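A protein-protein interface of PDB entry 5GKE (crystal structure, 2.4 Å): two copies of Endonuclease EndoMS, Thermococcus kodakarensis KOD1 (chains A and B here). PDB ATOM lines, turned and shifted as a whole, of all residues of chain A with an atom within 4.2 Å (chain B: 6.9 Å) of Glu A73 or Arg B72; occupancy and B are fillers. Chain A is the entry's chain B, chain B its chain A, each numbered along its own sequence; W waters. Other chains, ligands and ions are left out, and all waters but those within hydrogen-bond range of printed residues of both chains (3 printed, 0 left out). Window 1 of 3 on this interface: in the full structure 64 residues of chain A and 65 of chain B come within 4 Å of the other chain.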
ATOM      1  N   SER A  63       5.957  15.450 -13.732  1.00  0.00           N
ATOM      2  CA  SER A  63       5.503  14.235 -13.059  1.00  0.00           C
ATOM      3  C   SER A  63       6.553  13.139 -13.228  1.00  0.00           C
ATOM      4  O   SER A  63       7.075  12.920 -14.321  1.00  0.00           O
ATOM      5  CB  SER A  63       4.144  13.769 -13.608  1.00  0.00           C
ATOM      6  OG  SER A  63       3.151  14.782 -13.494  1.00  0.00           O
ATOM      7  N   LEU A  65       7.319   9.078 -12.158  1.00  0.00           N
ATOM      8  CA  LEU A  65       6.708   7.831 -11.676  1.00  0.00           C
ATOM      9  C   LEU A  65       7.695   6.683 -11.657  1.00  0.00           C
ATOM     10  O   LEU A  65       8.467   6.494 -12.606  1.00  0.00           O
ATOM     11  CB  LEU A  65       5.519   7.433 -12.551  1.00  0.00           C
ATOM     12  CG  LEU A  65       4.433   8.494 -12.741  1.00  0.00           C
ATOM     13  CD1 LEU A  65       3.496   8.096 -13.868  1.00  0.00           C
ATOM     14  CD2 LEU A  65       3.660   8.677 -11.463  1.00  0.00           C
ATOM     15  N   HIS A  67       7.429   2.594 -11.164  1.00  0.00           N
ATOM     16  CA  HIS A  67       6.516   1.458 -11.067  1.00  0.00           C
ATOM     17  C   HIS A  67       7.184   0.099 -10.922  1.00  0.00           C
ATOM     18  O   HIS A  67       8.011  -0.316 -11.751  1.00  0.00           O
ATOM     19  CB  HIS A  67       5.616   1.420 -12.294  1.00  0.00           C
ATOM     20  CG  HIS A  67       4.414   2.307 -12.192  1.00  0.00           C
ATOM     21  ND1 HIS A  67       3.347   2.016 -11.367  1.00  0.00           N
ATOM     22  CD2 HIS A  67       4.100   3.464 -12.818  1.00  0.00           C
ATOM     23  CE1 HIS A  67       2.433   2.957 -11.486  1.00  0.00           C
ATOM     24  NE2 HIS A  67       2.860   3.850 -12.363  1.00  0.00           N
ATOM     25  N   LYS A  71       0.930  -3.822  -8.383  1.00  0.00           N
ATOM     26  CA  LYS A  71      -0.042  -2.798  -8.022  1.00  0.00           C
ATOM     27  C   LYS A  71      -0.375  -1.717  -9.046  1.00  0.00           C
ATOM     28  O   LYS A  71       0.227  -1.635 -10.114  1.00  0.00           O
ATOM     29  CB  LYS A  71       0.481  -2.081  -6.760  1.00  0.00           C
ATOM     30  CG  LYS A  71       1.201  -2.994  -5.748  1.00  0.00           C
ATOM     31  CD  LYS A  71       0.506  -3.010  -4.396  1.00  0.00           C
ATOM     32  CE  LYS A  71       0.849  -4.259  -3.598  1.00  0.00           C
ATOM     33  NZ  LYS A  71       0.191  -5.455  -4.199  1.00  0.00           N
ATOM     34  N   ARG A  72      -1.236  -0.795  -8.620  1.00  0.00           N
ATOM     35  CA  ARG A  72      -1.748   0.258  -9.489  1.00  0.00           C
ATOM     36  C   ARG A  72      -0.894   1.505  -9.300  1.00  0.00           C
ATOM     37  O   ARG A  72      -0.575   2.207 -10.256  1.00  0.00           O
ATOM     38  CB  ARG A  72      -3.238   0.512  -9.231  1.00  0.00           C
ATOM     39  CG  ARG A  72      -3.948   1.379 -10.279  1.00  0.00           C
ATOM     40  CD  ARG A  72      -3.850   2.811  -9.835  1.00  0.00           C
ATOM     41  NE  ARG A  72      -4.755   3.727 -10.503  1.00  0.00           N
ATOM     42  CZ  ARG A  72      -5.125   4.876  -9.958  1.00  0.00           C
ATOM     43  NH1 ARG A  72      -4.667   5.185  -8.757  1.00  0.00           N
ATOM     44  NH2 ARG A  72      -5.954   5.700 -10.588  1.00  0.00           N
ATOM     45  N   GLU A  73      -0.553   1.755  -8.036  1.00  0.00           N
ATOM     46  CA  GLU A  73       0.247   2.893  -7.624  1.00  0.00           C
ATOM     47  C   GLU A  73       1.751   2.749  -7.942  1.00  0.00           C
ATOM     48  O   GLU A  73       2.322   1.669  -7.836  1.00  0.00           O
ATOM     49  CB  GLU A  73       0.070   3.119  -6.111  1.00  0.00           C
ATOM     50  CG  GLU A  73      -1.330   3.520  -5.703  1.00  0.00           C
ATOM     51  CD  GLU A  73      -1.856   4.626  -6.590  1.00  0.00           C
ATOM     52  OE1 GLU A  73      -2.786   4.352  -7.373  1.00  0.00           O
ATOM     53  OE2 GLU A  73      -1.315   5.758  -6.528  1.00  0.00           O
ATOM     54  N   PRO A  74       2.396   3.860  -8.285  1.00  0.00           N
ATOM     55  CA  PRO A  74       3.867   3.911  -8.277  1.00  0.00           C
ATOM     56  C   PRO A  74       4.425   3.689  -6.872  1.00  0.00           C
ATOM     57  O   PRO A  74       3.824   4.162  -5.916  1.00  0.00           O
ATOM     58  CB  PRO A  74       4.170   5.329  -8.751  1.00  0.00           C
ATOM     59  CG  PRO A  74       2.907   6.127  -8.383  1.00  0.00           C
ATOM     60  CD  PRO A  74       1.776   5.170  -8.587  1.00  0.00           C
ATOM     61  N   VAL A  75       5.540   2.975  -6.743  1.00  0.00           N
ATOM     62  CA  VAL A  75       6.172   2.797  -5.437  1.00  0.00           C
ATOM     63  C   VAL A  75       6.773   4.132  -4.939  1.00  0.00           C
ATOM     64  O   VAL A  75       6.795   4.424  -3.746  1.00  0.00           O
ATOM     65  CB  VAL A  75       7.268   1.701  -5.483  1.00  0.00           C
ATOM     66  CG1 VAL A  75       8.371   2.085  -6.466  1.00  0.00           C
ATOM     67  CG2 VAL A  75       7.856   1.486  -4.114  1.00  0.00           C
ATOM     68  N   TRP A  77       7.256   8.466  -6.454  1.00  0.00           N
ATOM     69  CA  TRP A  77       6.855   9.404  -7.469  1.00  0.00           C
ATOM     70  C   TRP A  77       7.204  10.826  -7.083  1.00  0.00           C
ATOM     71  O   TRP A  77       7.684  11.101  -5.999  1.00  0.00           O
ATOM     72  CB  TRP A  77       5.346   9.320  -7.699  1.00  0.00           C
ATOM     73  CG  TRP A  77       4.600   9.794  -6.512  1.00  0.00           C
ATOM     74  CD1 TRP A  77       4.103  11.046  -6.297  1.00  0.00           C
ATOM     75  CD2 TRP A  77       4.298   9.032  -5.338  1.00  0.00           C
ATOM     76  NE1 TRP A  77       3.488  11.103  -5.067  1.00  0.00           N
ATOM     77  CE2 TRP A  77       3.592   9.876  -4.461  1.00  0.00           C
ATOM     78  CE3 TRP A  77       4.539   7.706  -4.950  1.00  0.00           C
ATOM     79  CZ2 TRP A  77       3.130   9.443  -3.218  1.00  0.00           C
ATOM     80  CZ3 TRP A  77       4.080   7.278  -3.723  1.00  0.00           C
ATOM     81  CH2 TRP A  77       3.383   8.144  -2.869  1.00  0.00           C
ATOM     82  N   PRO A  80       3.332  16.753 -10.439  1.00  0.00           N
ATOM     83  CA  PRO A  80       3.536  17.787 -11.456  1.00  0.00           C
ATOM     84  C   PRO A  80       4.231  19.028 -10.910  1.00  0.00           C
ATOM     85  O   PRO A  80       3.936  19.464  -9.801  1.00  0.00           O
ATOM     86  CB  PRO A  80       2.111  18.128 -11.896  1.00  0.00           C
ATOM     87  CG  PRO A  80       1.335  16.880 -11.674  1.00  0.00           C
ATOM     88  CD  PRO A  80       1.974  16.173 -10.501  1.00  0.00           C
ATOM     89  N   LYS B  59       0.789  -4.548 -16.104  1.00  0.00           N
ATOM     90  CA  LYS B  59       1.573  -5.299 -15.154  1.00  0.00           C
ATOM     91  C   LYS B  59       1.089  -6.750 -15.065  1.00  0.00           C
ATOM     92  O   LYS B  59      -0.086  -7.026 -15.290  1.00  0.00           O
ATOM     93  CB  LYS B  59       1.494  -4.638 -13.779  1.00  0.00           C
ATOM     94  CG  LYS B  59       1.834  -3.174 -13.760  1.00  0.00           C
ATOM     95  CD  LYS B  59       2.098  -2.712 -12.345  1.00  0.00           C
ATOM     96  CE  LYS B  59       2.487  -1.254 -12.299  1.00  0.00           C
ATOM     97  NZ  LYS B  59       2.860  -0.866 -10.918  1.00  0.00           N
ATOM     98  N   SER B  63      -2.767  -5.028 -13.251  1.00  0.00           N
ATOM     99  CA  SER B  63      -2.809  -3.567 -13.232  1.00  0.00           C
ATOM    100  C   SER B  63      -2.596  -3.048 -14.646  1.00  0.00           C
ATOM    101  O   SER B  63      -1.744  -3.543 -15.394  1.00  0.00           O
ATOM    102  CB  SER B  63      -1.762  -2.997 -12.284  1.00  0.00           C
ATOM    103  OG  SER B  63      -1.862  -3.616 -11.018  1.00  0.00           O
ATOM    104  N   LEU B  65      -2.556   0.570 -16.869  1.00  0.00           N
ATOM    105  CA  LEU B  65      -2.449   2.033 -16.777  1.00  0.00           C
ATOM    106  C   LEU B  65      -2.350   2.693 -18.139  1.00  0.00           C
ATOM    107  O   LEU B  65      -1.536   2.299 -18.970  1.00  0.00           O
ATOM    108  CB  LEU B  65      -1.229   2.443 -15.954  1.00  0.00           C
ATOM    109  CG  LEU B  65      -0.964   1.706 -14.646  1.00  0.00           C
ATOM    110  CD1 LEU B  65       0.333   2.183 -14.050  1.00  0.00           C
ATOM    111  CD2 LEU B  65      -2.092   1.931 -13.677  1.00  0.00           C
ATOM    112  N   HIS B  67      -1.452   6.453 -19.528  1.00  0.00           N
ATOM    113  CA  HIS B  67      -0.937   7.752 -19.093  1.00  0.00           C
ATOM    114  C   HIS B  67      -0.864   8.737 -20.234  1.00  0.00           C
ATOM    115  O   HIS B  67      -0.343   8.419 -21.307  1.00  0.00           O
ATOM    116  CB  HIS B  67       0.448   7.626 -18.473  1.00  0.00           C
ATOM    117  CG  HIS B  67       0.447   7.275 -17.020  1.00  0.00           C
ATOM    118  ND1 HIS B  67       0.218   8.211 -16.029  1.00  0.00           N
ATOM    119  CD2 HIS B  67       0.681   6.106 -16.387  1.00  0.00           C
ATOM    120  CE1 HIS B  67       0.296   7.622 -14.852  1.00  0.00           C
ATOM    121  NE2 HIS B  67       0.578   6.343 -15.034  1.00  0.00           N
ATOM    122  N   LYS B  70       0.533  14.501 -19.220  1.00  0.00           N
ATOM    123  CA  LYS B  70       0.378  15.295 -18.018  1.00  0.00           C
ATOM    124  C   LYS B  70      -0.165  14.522 -16.822  1.00  0.00           C
ATOM    125  O   LYS B  70      -0.722  13.428 -16.929  1.00  0.00           O
ATOM    126  CB  LYS B  70      -0.523  16.503 -18.291  1.00  0.00           C
ATOM    127  CG  LYS B  70       0.137  17.538 -19.184  1.00  0.00           C
ATOM    128  CD  LYS B  70      -0.802  18.688 -19.514  1.00  0.00           C
ATOM    129  CE  LYS B  70      -0.232  19.549 -20.629  1.00  0.00           C
ATOM    130  NZ  LYS B  70       1.193  19.904 -20.382  1.00  0.00           N
ATOM    131  N   LYS B  71      -0.008  15.198 -15.695  1.00  0.00           N
ATOM    132  CA  LYS B  71      -0.330  14.839 -14.312  1.00  0.00           C
ATOM    133  C   LYS B  71       0.320  13.594 -13.744  1.00  0.00           C
ATOM    134  O   LYS B  71       1.093  12.922 -14.406  1.00  0.00           O
ATOM    135  CB  LYS B  71      -1.854  14.634 -14.192  1.00  0.00           C
ATOM    136  CG  LYS B  71      -2.728  15.597 -15.007  1.00  0.00           C
ATOM    137  CD  LYS B  71      -2.607  17.026 -14.493  1.00  0.00           C
ATOM    138  CE  LYS B  71      -3.239  17.166 -13.102  1.00  0.00           C
ATOM    139  NZ  LYS B  71      -3.172  18.556 -12.533  1.00  0.00           N
ATOM    140  N   ARG B  72      -0.116  13.200 -12.558  1.00  0.00           N
ATOM    141  CA  ARG B  72       0.543  12.082 -11.902  1.00  0.00           C
ATOM    142  C   ARG B  72      -0.308  10.830 -12.016  1.00  0.00           C
ATOM    143  O   ARG B  72       0.187   9.713 -11.930  1.00  0.00           O
ATOM    144  CB  ARG B  72       0.846  12.451 -10.450  1.00  0.00           C
ATOM    145  CG  ARG B  72       1.673  11.432  -9.674  1.00  0.00           C
ATOM    146  CD  ARG B  72       0.710  10.587  -8.895  1.00  0.00           C
ATOM    147  NE  ARG B  72       1.345   9.826  -7.853  1.00  0.00           N
ATOM    148  CZ  ARG B  72       0.680   9.011  -7.050  1.00  0.00           C
ATOM    149  NH1 ARG B  72      -0.631   8.873  -7.197  1.00  0.00           N
ATOM    150  NH2 ARG B  72       1.328   8.343  -6.107  1.00  0.00           N
ATOM    151  N   GLU B  73      -1.586  11.046 -12.296  1.00  0.00           N
ATOM    152  CA  GLU B  73      -2.565   9.982 -12.341  1.00  0.00           C
ATOM    153  C   GLU B  73      -2.727   9.491 -13.745  1.00  0.00           C
ATOM    154  O   GLU B  73      -2.700  10.279 -14.672  1.00  0.00           O
ATOM    155  CB  GLU B  73      -3.917  10.449 -11.808  1.00  0.00           C
ATOM    156  CG  GLU B  73      -3.916  10.729 -10.324  1.00  0.00           C
ATOM    157  CD  GLU B  73      -3.376   9.565  -9.543  1.00  0.00           C
ATOM    158  OE1 GLU B  73      -4.008   8.487  -9.585  1.00  0.00           O
ATOM    159  OE2 GLU B  73      -2.310   9.724  -8.905  1.00  0.00           O
ATOM    160  N   PRO B  74      -2.920   8.187 -13.905  1.00  0.00           N
ATOM    161  CA  PRO B  74      -3.274   7.748 -15.248  1.00  0.00           C
ATOM    162  C   PRO B  74      -4.680   8.263 -15.581  1.00  0.00           C
ATOM    163  O   PRO B  74      -5.515   8.378 -14.685  1.00  0.00           O
ATOM    164  CB  PRO B  74      -3.222   6.226 -15.124  1.00  0.00           C
ATOM    165  CG  PRO B  74      -3.685   5.984 -13.691  1.00  0.00           C
ATOM    166  CD  PRO B  74      -3.094   7.122 -12.896  1.00  0.00           C
ATOM    167  N   PRO B  80      -5.203  -4.144  -9.922  1.00  0.00           N
ATOM    168  CA  PRO B  80      -4.744  -5.539  -9.963  1.00  0.00           C
ATOM    169  C   PRO B  80      -5.913  -6.515 -10.010  1.00  0.00           C
ATOM    170  O   PRO B  80      -6.922  -6.245  -9.385  1.00  0.00           O
ATOM    171  CB  PRO B  80      -4.004  -5.704  -8.636  1.00  0.00           C
ATOM    172  CG  PRO B  80      -3.562  -4.376  -8.279  1.00  0.00           C
ATOM    173  CD  PRO B  80      -4.581  -3.405  -8.813  1.00  0.00           C
HETATM  174  O   HOH W   1       4.604   0.099  -8.381  1.00  0.00           O
HETATM  175  O   HOH W   2       0.787   5.639 -12.438  1.00  0.00           O
HETATM  176  O   HOH W   3      -1.600   6.525  -9.240  1.00  0.00           O
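NZ of Lys B59 sits at hydrogen-bond distance from ND1 of His A67 (3.0 Å).
O of Lys A71 is in hydrogen-bond range of NZ of Lys B59 (2.9 Å).
O of Lys A71 sits at hydrogen-bond distance from OG of Ser B63 (3.0 Å).
The backbone carbonyl oxygen (O) of Lys B71 lies within hydrogen-bond range of the side-chain hydroxyl (OG) of Ser A63 (2.9 Å).
The guanidinium group (NH1) of Arg B72 is in salt-bridge range of the side-chain carboxylate (OE2) of Glu A73, at 3.3 Å.
The side-chain carboxylate (OE1) of Glu B73 lies within salt-bridge range of the guanidinium group (NH1) of Arg A72 (3.5 Å).
OE2 of Glu B73 lies within salt-bridge range of NH1 of Arg B72.
The guanidinium group (NH1) of Arg A72 is in salt-bridge range of the side-chain carboxylate (OE1) of Glu A73 (2.5 Å).
Among the printed residues, merely in contact across the chains: Ser A63 with Arg B72, Leu A65 with His B67, Leu A65 with Arg B72, His A67 with Leu B65, Lys A71 with Pro B80, Arg A72 with Ser B63, Arg A72 with Leu B65, Arg A72 with Pro B74, Pro A74 with Arg B72, Trp A77 with Arg B72, Pro A80 with Lys B71 and Pro A80 with Arg B72.
Of the printed residues of chain B, Pro A74 touches Arg B72.
Of chain A, only Ser A63, Leu A65, Glu A73, Pro A74, Trp A77 and Pro A80 come within 4 Å of Arg B72.
Printed residues of chain A within 4 Å of Glu B73: Arg A72.
Printed residues of chain A within 4 Å of Pro B80: Lys A71.
The nearest residue of chain B that does not touch Glu A73 is Lys B59 (4.03 Å).
The nearest printed residue of chain A that does not touch Glu B73 is Glu A73 (4.7 Å).
Of the 10 printed residues of chain B, 9 touch a printed residue of chain A.
Printed residues of chain B that touch a printed residue of chain A: Lys B59, Ser B63, Leu B65, His B67, Lys B71, Arg B72, Glu B73, Pro B74 and Pro B80.
Hydrophobic or aromatic side chains of chain B that line the printed part of chain A: Leu B65, His B67, Pro B74 and Pro B80.
Printed residues of chain A that touch a printed residue of chain B: Ser A63, Leu A65, His A67, Lys A71, Arg A72, Glu A73, Pro A74, Trp A77 and Pro A80.
Hydrophobic or aromatic side chains of chain A within 4 Å of the printed part of chain B: Leu A65, His A67, Pro A74, Trp A77 and Pro A80.
Ser A63 touches Lys B71, and with the chains exchanged Lys A71 touches Ser B63.
Leu A65 touches His B67, and with the chains exchanged His A67 touches Leu B65.
Arg A72 touches Glu B73, and with the chains exchanged Glu A73 touches Arg B72.
Pro A80 touches Arg B72, but with the chains exchanged Arg A72 does not touch Pro B80 (4.2 Å).
Positions printed for both chains: 63, 65, 67, 71, 72, 73, 74 and 80.
Of the 18 pairs that touch across the chains among the printed residues, 14 have their exchanged pair printed and touching as well.
Water W2 bridges NE2 of His B67 (2.7 Å) and NE2 of His A67 (2.7 Å).
Water W1 lies within hydrogen-bond range of O of Glu A73 (2.8 Å), NZ of Lys B59 (3.2 Å) and N of Val A75 (3.4 Å).
Water W3 lies within hydrogen-bond range of the side-chain carboxylate of Glu A73 (2.8 Å), the side-chain carboxylate of Glu B73 (3.1 Å), the guanidinium group of Arg B72 (3.3 Å) and the guanidinium group of Arg A72 (3.4 Å).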
